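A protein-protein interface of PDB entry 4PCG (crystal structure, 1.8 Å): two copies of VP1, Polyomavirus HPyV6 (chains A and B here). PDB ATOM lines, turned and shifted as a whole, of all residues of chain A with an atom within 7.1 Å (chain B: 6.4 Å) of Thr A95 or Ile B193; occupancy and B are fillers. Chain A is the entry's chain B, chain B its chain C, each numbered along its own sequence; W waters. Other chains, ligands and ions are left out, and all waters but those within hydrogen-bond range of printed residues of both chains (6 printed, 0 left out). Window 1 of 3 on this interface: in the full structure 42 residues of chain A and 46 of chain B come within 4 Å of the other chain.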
ATOM      1  N   LEU A  92     -33.835  -3.060 -17.370  1.00  0.00           N
ATOM      2  CA  LEU A  92     -32.859  -2.936 -18.433  1.00  0.00           C
ATOM      3  C   LEU A  92     -31.458  -2.800 -17.865  1.00  0.00           C
ATOM      4  O   LEU A  92     -31.246  -2.130 -16.836  1.00  0.00           O
ATOM      5  CB  LEU A  92     -33.142  -1.698 -19.282  1.00  0.00           C
ATOM      6  CG  LEU A  92     -34.310  -1.732 -20.264  1.00  0.00           C
ATOM      7  CD1 LEU A  92     -34.314  -0.525 -21.185  1.00  0.00           C
ATOM      8  CD2 LEU A  92     -34.198  -3.004 -21.082  1.00  0.00           C
ATOM      9  N   ILE A  93     -30.505  -3.419 -18.560  1.00  0.00           N
ATOM     10  CA  ILE A  93     -29.100  -3.384 -18.202  1.00  0.00           C
ATOM     11  C   ILE A  93     -28.363  -2.515 -19.216  1.00  0.00           C
ATOM     12  O   ILE A  93     -28.320  -2.837 -20.398  1.00  0.00           O
ATOM     13  CB  ILE A  93     -28.475  -4.800 -18.194  1.00  0.00           C
ATOM     14  CG1 ILE A  93     -29.239  -5.686 -17.217  1.00  0.00           C
ATOM     15  CG2 ILE A  93     -27.021  -4.757 -17.803  1.00  0.00           C
ATOM     16  CD1 ILE A  93     -28.909  -7.143 -17.348  1.00  0.00           C
ATOM     17  N   PHE A  94     -27.785  -1.417 -18.740  1.00  0.00           N
ATOM     18  CA  PHE A  94     -27.123  -0.458 -19.636  1.00  0.00           C
ATOM     19  C   PHE A  94     -26.125   0.353 -18.836  1.00  0.00           C
ATOM     20  O   PHE A  94     -26.167   0.328 -17.604  1.00  0.00           O
ATOM     21  CB  PHE A  94     -28.161   0.447 -20.313  1.00  0.00           C
ATOM     22  CG  PHE A  94     -27.637   1.181 -21.524  1.00  0.00           C
ATOM     23  CD1 PHE A  94     -27.054   0.478 -22.570  1.00  0.00           C
ATOM     24  CD2 PHE A  94     -27.719   2.552 -21.601  1.00  0.00           C
ATOM     25  CE1 PHE A  94     -26.572   1.142 -23.686  1.00  0.00           C
ATOM     26  CE2 PHE A  94     -27.248   3.218 -22.722  1.00  0.00           C
ATOM     27  CZ  PHE A  94     -26.661   2.504 -23.747  1.00  0.00           C
ATOM     28  N   THR A  95     -25.225   1.057 -19.544  1.00  0.00           N
ATOM     29  CA  THR A  95     -24.273   1.992 -18.968  1.00  0.00           C
ATOM     30  C   THR A  95     -24.288   3.281 -19.817  1.00  0.00           C
ATOM     31  O   THR A  95     -24.636   3.233 -20.996  1.00  0.00           O
ATOM     32  CB  THR A  95     -22.843   1.428 -19.047  1.00  0.00           C
ATOM     33  OG1 THR A  95     -22.569   1.102 -20.413  1.00  0.00           O
ATOM     34  CG2 THR A  95     -22.706   0.180 -18.172  1.00  0.00           C
ATOM     35  N   PRO A  96     -23.924   4.427 -19.235  1.00  0.00           N
ATOM     36  CA  PRO A  96     -23.857   5.649 -20.030  1.00  0.00           C
ATOM     37  C   PRO A  96     -22.804   5.550 -21.122  1.00  0.00           C
ATOM     38  O   PRO A  96     -21.723   5.027 -20.881  1.00  0.00           O
ATOM     39  CB  PRO A  96     -23.492   6.727 -19.008  1.00  0.00           C
ATOM     40  CG  PRO A  96     -22.873   5.968 -17.880  1.00  0.00           C
ATOM     41  CD  PRO A  96     -23.551   4.665 -17.832  1.00  0.00           C
ATOM     42  N   GLN A  97     -23.159   6.029 -22.318  1.00  0.00           N
ATOM     43  CA  GLN A  97     -22.273   6.045 -23.452  1.00  0.00           C
ATOM     44  C   GLN A  97     -21.801   7.482 -23.689  1.00  0.00           C
ATOM     45  O   GLN A  97     -22.610   8.388 -23.872  1.00  0.00           O
ATOM     46  CB  GLN A  97     -23.000   5.510 -24.695  1.00  0.00           C
ATOM     47  CG  GLN A  97     -23.625   4.145 -24.512  1.00  0.00           C
ATOM     48  CD  GLN A  97     -22.605   3.068 -24.226  1.00  0.00           C
ATOM     49  OE1 GLN A  97     -21.716   2.806 -25.045  1.00  0.00           O
ATOM     50  NE2 GLN A  97     -22.725   2.419 -23.067  1.00  0.00           N
ATOM     51  N   LEU A  98     -20.495   7.692 -23.626  1.00  0.00           N
ATOM     52  CA  LEU A  98     -19.911   8.993 -23.951  1.00  0.00           C
ATOM     53  C   LEU A  98     -19.072   8.795 -25.215  1.00  0.00           C
ATOM     54  O   LEU A  98     -19.642   8.669 -26.306  1.00  0.00           O
ATOM     55  CB  LEU A  98     -19.105   9.569 -22.786  1.00  0.00           C
ATOM     56  CG  LEU A  98     -19.911  10.362 -21.756  1.00  0.00           C
ATOM     57  CD1 LEU A  98     -20.981   9.483 -21.113  1.00  0.00           C
ATOM     58  CD2 LEU A  98     -18.973  10.954 -20.714  1.00  0.00           C
ATOM     59  N   SER A 100     -17.518   6.242 -26.281  1.00  0.00           N
ATOM     60  CA  SER A 100     -17.761   4.939 -26.918  1.00  0.00           C
ATOM     61  C   SER A 100     -18.613   5.063 -28.181  1.00  0.00           C
ATOM     62  O   SER A 100     -18.596   4.156 -29.031  1.00  0.00           O
ATOM     63  CB  SER A 100     -18.473   3.965 -25.967  1.00  0.00           C
ATOM     64  OG  SER A 100     -19.835   4.336 -25.779  1.00  0.00           O
ATOM     65  N   VAL A 113     -25.493   8.383 -26.947  1.00  0.00           N
ATOM     66  CA  VAL A 113     -26.566   7.718 -27.668  1.00  0.00           C
ATOM     67  C   VAL A 113     -27.764   8.650 -27.732  1.00  0.00           C
ATOM     68  O   VAL A 113     -28.143   9.305 -26.741  1.00  0.00           O
ATOM     69  CB  VAL A 113     -26.907   6.333 -27.073  1.00  0.00           C
ATOM     70  CG1 VAL A 113     -27.105   6.393 -25.585  1.00  0.00           C
ATOM     71  CG2 VAL A 113     -28.124   5.731 -27.778  1.00  0.00           C
ATOM     72  N   TYR A 119     -38.984   0.699 -26.050  1.00  0.00           N
ATOM     73  CA  TYR A 119     -38.780  -0.096 -24.841  1.00  0.00           C
ATOM     74  C   TYR A 119     -40.004  -1.026 -24.765  1.00  0.00           C
ATOM     75  O   TYR A 119     -41.112  -0.541 -24.790  1.00  0.00           O
ATOM     76  CB  TYR A 119     -38.769   0.799 -23.604  1.00  0.00           C
ATOM     77  CG  TYR A 119     -37.796   1.969 -23.704  1.00  0.00           C
ATOM     78  CD1 TYR A 119     -36.498   1.822 -23.277  1.00  0.00           C
ATOM     79  CD2 TYR A 119     -38.172   3.184 -24.246  1.00  0.00           C
ATOM     80  CE1 TYR A 119     -35.591   2.861 -23.376  1.00  0.00           C
ATOM     81  CE2 TYR A 119     -37.262   4.235 -24.343  1.00  0.00           C
ATOM     82  CZ  TYR A 119     -35.972   4.064 -23.909  1.00  0.00           C
ATOM     83  OH  TYR A 119     -35.029   5.090 -23.997  1.00  0.00           O
ATOM     84  N   PRO A 201     -32.294   9.119 -24.848  1.00  0.00           N
ATOM     85  CA  PRO A 201     -32.983   8.089 -24.084  1.00  0.00           C
ATOM     86  C   PRO A 201     -32.886   8.312 -22.575  1.00  0.00           C
ATOM     87  O   PRO A 201     -31.987   8.989 -22.094  1.00  0.00           O
ATOM     88  CB  PRO A 201     -32.256   6.805 -24.471  1.00  0.00           C
ATOM     89  CG  PRO A 201     -30.866   7.293 -24.781  1.00  0.00           C
ATOM     90  CD  PRO A 201     -31.035   8.628 -25.424  1.00  0.00           C
ATOM     91  N   VAL A 202     -33.858   7.752 -21.849  1.00  0.00           N
ATOM     92  CA  VAL A 202     -33.868   7.779 -20.389  1.00  0.00           C
ATOM     93  C   VAL A 202     -34.137   6.344 -19.979  1.00  0.00           C
ATOM     94  O   VAL A 202     -35.144   5.753 -20.397  1.00  0.00           O
ATOM     95  CB  VAL A 202     -34.938   8.711 -19.801  1.00  0.00           C
ATOM     96  CG1 VAL A 202     -34.899   8.666 -18.252  1.00  0.00           C
ATOM     97  CG2 VAL A 202     -34.730  10.112 -20.284  1.00  0.00           C
ATOM     98  N   VAL A 203     -33.192   5.745 -19.262  1.00  0.00           N
ATOM     99  CA  VAL A 203     -33.310   4.362 -18.776  1.00  0.00           C
ATOM    100  C   VAL A 203     -33.283   4.380 -17.248  1.00  0.00           C
ATOM    101  O   VAL A 203     -32.273   4.758 -16.667  1.00  0.00           O
ATOM    102  CB  VAL A 203     -32.149   3.501 -19.312  1.00  0.00           C
ATOM    103  CG1 VAL A 203     -32.137   2.102 -18.688  1.00  0.00           C
ATOM    104  CG2 VAL A 203     -32.213   3.378 -20.835  1.00  0.00           C
ATOM    105  N   SER A 204     -34.383   3.995 -16.591  1.00  0.00           N
ATOM    106  CA  SER A 204     -34.400   3.888 -15.155  1.00  0.00           C
ATOM    107  C   SER A 204     -34.360   2.404 -14.800  1.00  0.00           C
ATOM    108  O   SER A 204     -34.944   1.588 -15.519  1.00  0.00           O
ATOM    109  CB  SER A 204     -35.667   4.548 -14.599  1.00  0.00           C
ATOM    110  OG  SER A 204     -35.652   5.948 -14.828  1.00  0.00           O
ATOM    111  N   PHE A 205     -33.674   2.056 -13.710  1.00  0.00           N
ATOM    112  CA  PHE A 205     -33.535   0.662 -13.325  1.00  0.00           C
ATOM    113  C   PHE A 205     -33.292   0.563 -11.818  1.00  0.00           C
ATOM    114  O   PHE A 205     -32.947   1.545 -11.162  1.00  0.00           O
ATOM    115  CB  PHE A 205     -32.414  -0.020 -14.138  1.00  0.00           C
ATOM    116  CG  PHE A 205     -31.069   0.628 -13.981  1.00  0.00           C
ATOM    117  CD1 PHE A 205     -30.750   1.763 -14.692  1.00  0.00           C
ATOM    118  CD2 PHE A 205     -30.122   0.108 -13.108  1.00  0.00           C
ATOM    119  CE1 PHE A 205     -29.515   2.373 -14.548  1.00  0.00           C
ATOM    120  CE2 PHE A 205     -28.884   0.732 -12.944  1.00  0.00           C
ATOM    121  CZ  PHE A 205     -28.581   1.859 -13.685  1.00  0.00           C
ATOM    122  N   LEU A 236     -32.316   2.100 -27.848  1.00  0.00           N
ATOM    123  CA  LEU A 236     -32.073   3.334 -27.112  1.00  0.00           C
ATOM    124  C   LEU A 236     -31.680   4.525 -27.961  1.00  0.00           C
ATOM    125  O   LEU A 236     -31.687   5.657 -27.475  1.00  0.00           O
ATOM    126  CB  LEU A 236     -30.970   3.068 -26.067  1.00  0.00           C
ATOM    127  CG  LEU A 236     -31.253   1.909 -25.107  1.00  0.00           C
ATOM    128  CD1 LEU A 236     -30.131   1.747 -24.084  1.00  0.00           C
ATOM    129  CD2 LEU A 236     -32.565   2.133 -24.424  1.00  0.00           C
ATOM    130  N   GLN A 258     -28.160   1.402 -31.276  1.00  0.00           N
ATOM    131  CA  GLN A 258     -27.742   0.987 -29.940  1.00  0.00           C
ATOM    132  C   GLN A 258     -28.939   0.379 -29.198  1.00  0.00           C
ATOM    133  O   GLN A 258     -29.971   1.040 -29.032  1.00  0.00           O
ATOM    134  CB  GLN A 258     -27.245   2.206 -29.143  1.00  0.00           C
ATOM    135  CG  GLN A 258     -26.914   1.910 -27.692  1.00  0.00           C
ATOM    136  CD  GLN A 258     -25.589   1.216 -27.556  1.00  0.00           C
ATOM    137  OE1 GLN A 258     -24.560   1.814 -27.828  1.00  0.00           O
ATOM    138  NE2 GLN A 258     -25.593  -0.034 -27.137  1.00  0.00           N
ATOM    139  N   PHE A 261     -27.994  -3.662 -23.135  1.00  0.00           N
ATOM    140  CA  PHE A 261     -27.161  -4.876 -23.062  1.00  0.00           C
ATOM    141  C   PHE A 261     -27.967  -6.131 -22.738  1.00  0.00           C
ATOM    142  O   PHE A 261     -27.534  -7.245 -22.990  1.00  0.00           O
ATOM    143  CB  PHE A 261     -26.042  -4.729 -22.040  1.00  0.00           C
ATOM    144  CG  PHE A 261     -25.121  -3.570 -22.293  1.00  0.00           C
ATOM    145  CD1 PHE A 261     -24.669  -3.278 -23.577  1.00  0.00           C
ATOM    146  CD2 PHE A 261     -24.661  -2.812 -21.254  1.00  0.00           C
ATOM    147  CE1 PHE A 261     -23.796  -2.227 -23.802  1.00  0.00           C
ATOM    148  CE2 PHE A 261     -23.783  -1.752 -21.454  1.00  0.00           C
ATOM    149  CZ  PHE A 261     -23.345  -1.449 -22.737  1.00  0.00           C
ATOM    150  N   TYR B  61     -17.378   4.363  -9.912  1.00  0.00           N
ATOM    151  CA  TYR B  61     -18.227   4.291  -8.736  1.00  0.00           C
ATOM    152  C   TYR B  61     -17.435   4.750  -7.515  1.00  0.00           C
ATOM    153  O   TYR B  61     -16.213   4.525  -7.426  1.00  0.00           O
ATOM    154  CB  TYR B  61     -18.676   2.866  -8.499  1.00  0.00           C
ATOM    155  CG  TYR B  61     -19.736   2.378  -9.454  1.00  0.00           C
ATOM    156  CD1 TYR B  61     -21.074   2.698  -9.261  1.00  0.00           C
ATOM    157  CD2 TYR B  61     -19.406   1.590 -10.529  1.00  0.00           C
ATOM    158  CE1 TYR B  61     -22.045   2.226 -10.119  1.00  0.00           C
ATOM    159  CE2 TYR B  61     -20.376   1.101 -11.385  1.00  0.00           C
ATOM    160  CZ  TYR B  61     -21.697   1.442 -11.178  1.00  0.00           C
ATOM    161  OH  TYR B  61     -22.665   0.957 -12.048  1.00  0.00           O
ATOM    162  N   GLN B 117     -25.878  11.533 -18.637  1.00  0.00           N
ATOM    163  CA  GLN B 117     -25.935  11.556 -17.211  1.00  0.00           C
ATOM    164  C   GLN B 117     -26.124  10.158 -16.650  1.00  0.00           C
ATOM    165  O   GLN B 117     -26.641   9.274 -17.329  1.00  0.00           O
ATOM    166  CB  GLN B 117     -27.105  12.410 -16.749  1.00  0.00           C
ATOM    167  CG  GLN B 117     -27.081  13.836 -17.281  1.00  0.00           C
ATOM    168  CD  GLN B 117     -28.453  14.425 -17.465  1.00  0.00           C
ATOM    169  OE1 GLN B 117     -29.352  14.209 -16.649  1.00  0.00           O
ATOM    170  NE2 GLN B 117     -28.625  15.197 -18.535  1.00  0.00           N
ATOM    171  N   MET B 118     -25.717   9.993 -15.412  1.00  0.00           N
ATOM    172  CA  MET B 118     -26.060   8.818 -14.623  1.00  0.00           C
ATOM    173  C   MET B 118     -26.239   9.210 -13.180  1.00  0.00           C
ATOM    174  O   MET B 118     -25.410   9.903 -12.609  1.00  0.00           O
ATOM    175  CB  MET B 118     -25.000   7.733 -14.753  1.00  0.00           C
ATOM    176  CG  MET B 118     -25.328   6.488 -13.912  1.00  0.00           C
ATOM    177  SD  MET B 118     -24.192   5.148 -14.262  1.00  0.00           S
ATOM    178  CE  MET B 118     -24.540   3.973 -12.943  1.00  0.00           C
ATOM    179  N   TYR B 119     -27.318   8.739 -12.581  1.00  0.00           N
ATOM    180  CA  TYR B 119     -27.623   8.981 -11.181  1.00  0.00           C
ATOM    181  C   TYR B 119     -27.813   7.596 -10.579  1.00  0.00           C
ATOM    182  O   TYR B 119     -28.629   6.837 -11.057  1.00  0.00           O
ATOM    183  CB  TYR B 119     -28.920   9.786 -11.016  1.00  0.00           C
ATOM    184  CG  TYR B 119     -28.941  11.060 -11.799  1.00  0.00           C
ATOM    185  CD1 TYR B 119     -28.469  12.234 -11.253  1.00  0.00           C
ATOM    186  CD2 TYR B 119     -29.427  11.094 -13.094  1.00  0.00           C
ATOM    187  CE1 TYR B 119     -28.465  13.418 -11.996  1.00  0.00           C
ATOM    188  CE2 TYR B 119     -29.412  12.267 -13.844  1.00  0.00           C
ATOM    189  CZ  TYR B 119     -28.934  13.431 -13.292  1.00  0.00           C
ATOM    190  OH  TYR B 119     -28.923  14.611 -14.052  1.00  0.00           O
ATOM    191  N   ILE B 131     -21.806  -6.077 -13.755  1.00  0.00           N
ATOM    192  CA  ILE B 131     -21.518  -6.738 -14.996  1.00  0.00           C
ATOM    193  C   ILE B 131     -20.718  -5.741 -15.819  1.00  0.00           C
ATOM    194  O   ILE B 131     -21.109  -4.582 -15.899  1.00  0.00           O
ATOM    195  CB  ILE B 131     -22.813  -7.045 -15.766  1.00  0.00           C
ATOM    196  CG1 ILE B 131     -23.766  -7.880 -14.915  1.00  0.00           C
ATOM    197  CG2 ILE B 131     -22.526  -7.774 -17.075  1.00  0.00           C
ATOM    198  CD1 ILE B 131     -25.139  -7.996 -15.540  1.00  0.00           C
ATOM    199  N   ILE B 133     -19.166  -4.603 -19.415  1.00  0.00           N
ATOM    200  CA  ILE B 133     -19.331  -4.784 -20.859  1.00  0.00           C
ATOM    201  C   ILE B 133     -18.658  -3.671 -21.655  1.00  0.00           C
ATOM    202  O   ILE B 133     -18.822  -2.496 -21.358  1.00  0.00           O
ATOM    203  CB  ILE B 133     -20.831  -4.855 -21.224  1.00  0.00           C
ATOM    204  CG1 ILE B 133     -21.459  -6.081 -20.541  1.00  0.00           C
ATOM    205  CG2 ILE B 133     -21.041  -4.941 -22.743  1.00  0.00           C
ATOM    206  CD1 ILE B 133     -22.959  -6.144 -20.662  1.00  0.00           C
ATOM    207  N   PRO B 135     -18.792  -1.688 -24.862  1.00  0.00           N
ATOM    208  CA  PRO B 135     -19.848  -1.424 -25.833  1.00  0.00           C
ATOM    209  C   PRO B 135     -19.431  -1.499 -27.299  1.00  0.00           C
ATOM    210  O   PRO B 135     -20.290  -1.596 -28.181  1.00  0.00           O
ATOM    211  CB  PRO B 135     -20.267  -0.007 -25.508  1.00  0.00           C
ATOM    212  CG  PRO B 135     -19.156   0.602 -24.758  1.00  0.00           C
ATOM    213  CD  PRO B 135     -18.409  -0.489 -24.094  1.00  0.00           C
ATOM    214  N   PRO B 173     -15.099   1.979 -13.807  1.00  0.00           N
ATOM    215  CA  PRO B 173     -15.735   3.058 -14.547  1.00  0.00           C
ATOM    216  C   PRO B 173     -17.192   2.803 -14.854  1.00  0.00           C
ATOM    217  O   PRO B 173     -17.562   1.716 -15.252  1.00  0.00           O
ATOM    218  CB  PRO B 173     -14.917   3.140 -15.845  1.00  0.00           C
ATOM    219  CG  PRO B 173     -14.282   1.812 -16.006  1.00  0.00           C
ATOM    220  CD  PRO B 173     -14.055   1.308 -14.599  1.00  0.00           C
ATOM    221  N   ILE B 174     -18.024   3.810 -14.662  1.00  0.00           N
ATOM    222  CA  ILE B 174     -19.448   3.679 -14.947  1.00  0.00           C
ATOM    223  C   ILE B 174     -19.739   3.495 -16.443  1.00  0.00           C
ATOM    224  O   ILE B 174     -20.815   3.023 -16.811  1.00  0.00           O
ATOM    225  CB  ILE B 174     -20.255   4.861 -14.387  1.00  0.00           C
ATOM    226  CG1 ILE B 174     -19.909   6.162 -15.113  1.00  0.00           C
ATOM    227  CG2 ILE B 174     -20.068   4.960 -12.887  1.00  0.00           C
ATOM    228  CD1 ILE B 174     -20.808   7.325 -14.712  1.00  0.00           C
ATOM    229  N   GLU B 175     -18.780   3.849 -17.305  1.00  0.00           N
ATOM    230  CA  GLU B 175     -18.921   3.594 -18.748  1.00  0.00           C
ATOM    231  C   GLU B 175     -18.735   2.102 -19.133  1.00  0.00           C
ATOM    232  O   GLU B 175     -18.917   1.739 -20.292  1.00  0.00           O
ATOM    233  CB  GLU B 175     -17.986   4.508 -19.560  1.00  0.00           C
ATOM    234  CG  GLU B 175     -18.389   5.974 -19.490  1.00  0.00           C
ATOM    235  CD  GLU B 175     -17.264   6.899 -19.914  1.00  0.00           C
ATOM    236  OE1 GLU B 175     -17.052   7.002 -21.141  1.00  0.00           O
ATOM    237  OE2 GLU B 175     -16.586   7.483 -19.017  1.00  0.00           O
ATOM    238  N   ILE B 176     -18.424   1.245 -18.163  1.00  0.00           N
ATOM    239  CA  ILE B 176     -18.252  -0.192 -18.397  1.00  0.00           C
ATOM    240  C   ILE B 176     -19.155  -1.052 -17.480  1.00  0.00           C
ATOM    241  O   ILE B 176     -19.696  -2.061 -17.937  1.00  0.00           O
ATOM    242  CB  ILE B 176     -16.782  -0.582 -18.141  1.00  0.00           C
ATOM    243  CG1 ILE B 176     -15.854   0.107 -19.172  1.00  0.00           C
ATOM    244  CG2 ILE B 176     -16.600  -2.101 -18.147  1.00  0.00           C
ATOM    245  CD1 ILE B 176     -16.040  -0.412 -20.594  1.00  0.00           C
ATOM    246  N   TRP B 177     -19.312  -0.656 -16.215  1.00  0.00           N
ATOM    247  CA  TRP B 177     -19.889  -1.547 -15.175  1.00  0.00           C
ATOM    248  C   TRP B 177     -21.301  -1.177 -14.743  1.00  0.00           C
ATOM    249  O   TRP B 177     -21.523  -0.092 -14.233  1.00  0.00           O
ATOM    250  CB  TRP B 177     -18.987  -1.605 -13.929  1.00  0.00           C
ATOM    251  CG  TRP B 177     -17.636  -2.131 -14.240  1.00  0.00           C
ATOM    252  CD1 TRP B 177     -16.529  -1.381 -14.580  1.00  0.00           C
ATOM    253  CD2 TRP B 177     -17.213  -3.496 -14.295  1.00  0.00           C
ATOM    254  NE1 TRP B 177     -15.484  -2.179 -14.855  1.00  0.00           N
ATOM    255  CE2 TRP B 177     -15.849  -3.489 -14.679  1.00  0.00           C
ATOM    256  CE3 TRP B 177     -17.838  -4.718 -14.063  1.00  0.00           C
ATOM    257  CZ2 TRP B 177     -15.115  -4.652 -14.839  1.00  0.00           C
ATOM    258  CZ3 TRP B 177     -17.102  -5.878 -14.225  1.00  0.00           C
ATOM    259  CH2 TRP B 177     -15.761  -5.849 -14.598  1.00  0.00           C
ATOM    260  N   SER B 178     -22.242  -2.107 -14.934  1.00  0.00           N
ATOM    261  CA  SER B 178     -23.658  -1.929 -14.573  1.00  0.00           C
ATOM    262  C   SER B 178     -24.029  -2.859 -13.416  1.00  0.00           C
ATOM    263  O   SER B 178     -23.542  -3.985 -13.346  1.00  0.00           O
ATOM    264  CB  SER B 178     -24.537  -2.270 -15.784  1.00  0.00           C
ATOM    265  OG  SER B 178     -25.910  -1.977 -15.586  1.00  0.00           O
ATOM    266  N   GLY B 191     -31.012   3.379 -10.249  1.00  0.00           N
ATOM    267  CA  GLY B 191     -30.225   4.116 -11.220  1.00  0.00           C
ATOM    268  C   GLY B 191     -31.051   4.728 -12.324  1.00  0.00           C
ATOM    269  O   GLY B 191     -32.115   4.256 -12.669  1.00  0.00           O
ATOM    270  N   ARG B 192     -30.535   5.813 -12.885  1.00  0.00           N
ATOM    271  CA  ARG B 192     -31.149   6.439 -14.019  1.00  0.00           C
ATOM    272  C   ARG B 192     -30.033   6.905 -14.933  1.00  0.00           C
ATOM    273  O   ARG B 192     -29.116   7.605 -14.485  1.00  0.00           O
ATOM    274  CB  ARG B 192     -32.000   7.628 -13.588  1.00  0.00           C
ATOM    275  CG  ARG B 192     -32.711   8.304 -14.754  1.00  0.00           C
ATOM    276  CD  ARG B 192     -33.876   9.173 -14.309  1.00  0.00           C
ATOM    277  NE  ARG B 192     -33.340  10.376 -13.688  1.00  0.00           N
ATOM    278  CZ  ARG B 192     -33.267  10.623 -12.381  1.00  0.00           C
ATOM    279  NH1 ARG B 192     -33.731   9.755 -11.467  1.00  0.00           N
ATOM    280  NH2 ARG B 192     -32.715  11.769 -11.986  1.00  0.00           N
ATOM    281  N   ILE B 193     -30.110   6.486 -16.192  1.00  0.00           N
ATOM    282  CA  ILE B 193     -29.175   6.951 -17.237  1.00  0.00           C
ATOM    283  C   ILE B 193     -29.929   7.804 -18.239  1.00  0.00           C
ATOM    284  O   ILE B 193     -31.014   7.444 -18.709  1.00  0.00           O
ATOM    285  CB  ILE B 193     -28.546   5.744 -17.943  1.00  0.00           C
ATOM    286  CG1 ILE B 193     -27.639   4.986 -16.971  1.00  0.00           C
ATOM    287  CG2 ILE B 193     -27.784   6.145 -19.203  1.00  0.00           C
ATOM    288  CD1 ILE B 193     -27.417   3.570 -17.412  1.00  0.00           C
ATOM    289  N   VAL B 194     -29.310   8.920 -18.640  1.00  0.00           N
ATOM    290  CA  VAL B 194     -29.869   9.815 -19.623  1.00  0.00           C
ATOM    291  C   VAL B 194     -28.807   9.971 -20.706  1.00  0.00           C
ATOM    292  O   VAL B 194     -27.627  10.208 -20.412  1.00  0.00           O
ATOM    293  CB  VAL B 194     -30.179  11.194 -19.004  1.00  0.00           C
ATOM    294  CG1 VAL B 194     -30.808  12.128 -20.021  1.00  0.00           C
ATOM    295  CG2 VAL B 194     -31.091  11.033 -17.774  1.00  0.00           C
ATOM    296  N   GLY B 195     -29.214   9.791 -21.951  1.00  0.00           N
ATOM    297  CA  GLY B 195     -28.290   9.888 -23.068  1.00  0.00           C
ATOM    298  C   GLY B 195     -28.249  11.290 -23.627  1.00  0.00           C
ATOM    299  O   GLY B 195     -28.610  12.249 -22.945  1.00  0.00           O
HETATM  300  O   HOH W   1     -19.662   3.510 -22.435  1.00  0.00           O
HETATM  301  O   HOH W   2     -22.904  -1.413 -27.113  1.00  0.00           O
HETATM  302  O   HOH W   3     -20.472  -0.143 -21.311  1.00  0.00           O
HETATM  303  O   HOH W   4     -28.733  -0.779 -16.097  1.00  0.00           O
HETATM  304  O   HOH W   5     -35.994   7.448 -12.473  1.00  0.00           O
HETATM  305  O   HOH W   6     -18.316   5.822 -23.257  1.00  0.00           O
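O of Ile A93 is in hydrogen-bond range of N of Phe A261.
O of Thr A95 lies within hydrogen-bond range of NE2 of Gln A97.
The side-chain hydroxyl of Ser A100 lies within hydrogen-bond range of the side-chain amide oxygen of Gln A97 (2.5 Å).
O of Val B194 lies within hydrogen-bond range of N of Gln B117 (2.8 Å).
The backbone NH of Arg B192 lies within hydrogen-bond range of the backbone carbonyl oxygen of Tyr B119.
O of Ile B176 is in hydrogen-bond range of N of Ile B133 (3.0 Å).
Of the 18 printed residues of chain A, 14 touch a printed residue of chain B.
Hydrophobic or aromatic side chains of chain A that line the printed part of chain B: Ile A93, Pro A96, Leu A98, Pro A201, Phe A205 and Phe A261.
Among the printed residues, 28 pairs touch across the chains.
Position printed for both chains: 119.
Of the 28 pairs that touch across the chains among the printed residues, none has its exchanged pair printed and touching as well.
Water W3 lies within hydrogen-bond range of the side-chain hydroxyl (OG1) of Thr A95 (2.6 Å), the backbone carbonyl oxygen (O) of Glu B175 (2.6 Å) and the backbone carbonyl oxygen (O) of Ile B133 (2.9 Å).
Water W2 bridges O of Pro B135 and NE2 of Gln A258.
Water W1 lies within hydrogen-bond range of the backbone carbonyl oxygen of Glu B175 (2.9 Å), the backbone carbonyl oxygen of Pro A96 (3.0 Å), the side-chain amide nitrogen of Gln A97 (3.3 Å) and the side-chain hydroxyl of Ser A100 (3.4 Å).
Water W4 lies within hydrogen-bond range of the backbone NH of Phe A94 (2.9 Å), the backbone carbonyl oxygen of Leu A92 (2.9 Å) and the side-chain hydroxyl of Ser B178 (3.1 Å).
Printed residues of chain B within 4 Å of Thr A95: Ile B174, Glu B175, Ile B176, Trp B177, Ser B178 and Ile B193.
Printed residues of chain A within 4 Å of Ile B193: Phe A94, Thr A95, Pro A201, Val A202, Val A203 and Phe A205.
Of the printed residues of chain B, Val A203 touches Arg B192 (3.3 Å) and Ile B193 (2.8 Å).
Of the printed residues of chain A, Glu B175 touches Thr A95, Pro A96 and Leu A98.
Printed residues of chain A within 4 Å of Val B194: Pro A201 (3.4 Å).
Tyr A119 touches none of the printed residues of chain B.
Ile B131 touches none of the printed residues of chain A.
The nearest printed residue of chain B that does not touch Thr A95 is Ile B133 (5.3 Å).
Among the printed residues, merely in contact across the chains: Gln A97 with Pro B135, Val A202 with Ile B193, Val A203 with Arg B192, Pro A96 with Ile B174, Pro A201 with Val B194, Ser A204 with Gly B191, Thr A95 with Ile B174, Phe A94 with Ile B193, Ser A100 with Pro B135, Pro A96 with Met B118, Phe A261 with Ile B133, Leu A98 with Glu B175, Val A113 with Gly B195, Thr A95 with Glu B175, Ser A204 with Arg B192, Ile A93 with Ser B178, Pro A96 with Glu B175, Phe A205 with Ile B193, Thr A95 with Ile B176, Pro A201 with Ile B193, Thr A95 with Ile B193, Thr A95 with Ser B178, Thr A95 with Trp B177 and Phe A205 with Arg B192.
The side-chain hydroxyl of Ser B178 sits at hydrogen-bond distance from the backbone carbonyl oxygen of Phe A94, 3.1 Å away.
The backbone carbonyl oxygen (O) of Pro A201 lies within hydrogen-bond range of the backbone NH (N) of Gly B195, at 2.9 Å.
The backbone carbonyl oxygen (O) of Val A203 sits at hydrogen-bond distance from the backbone NH (N) of Ile B193.
O of Phe A205 lies within hydrogen-bond range of N of Gly B191 (2.8 Å).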
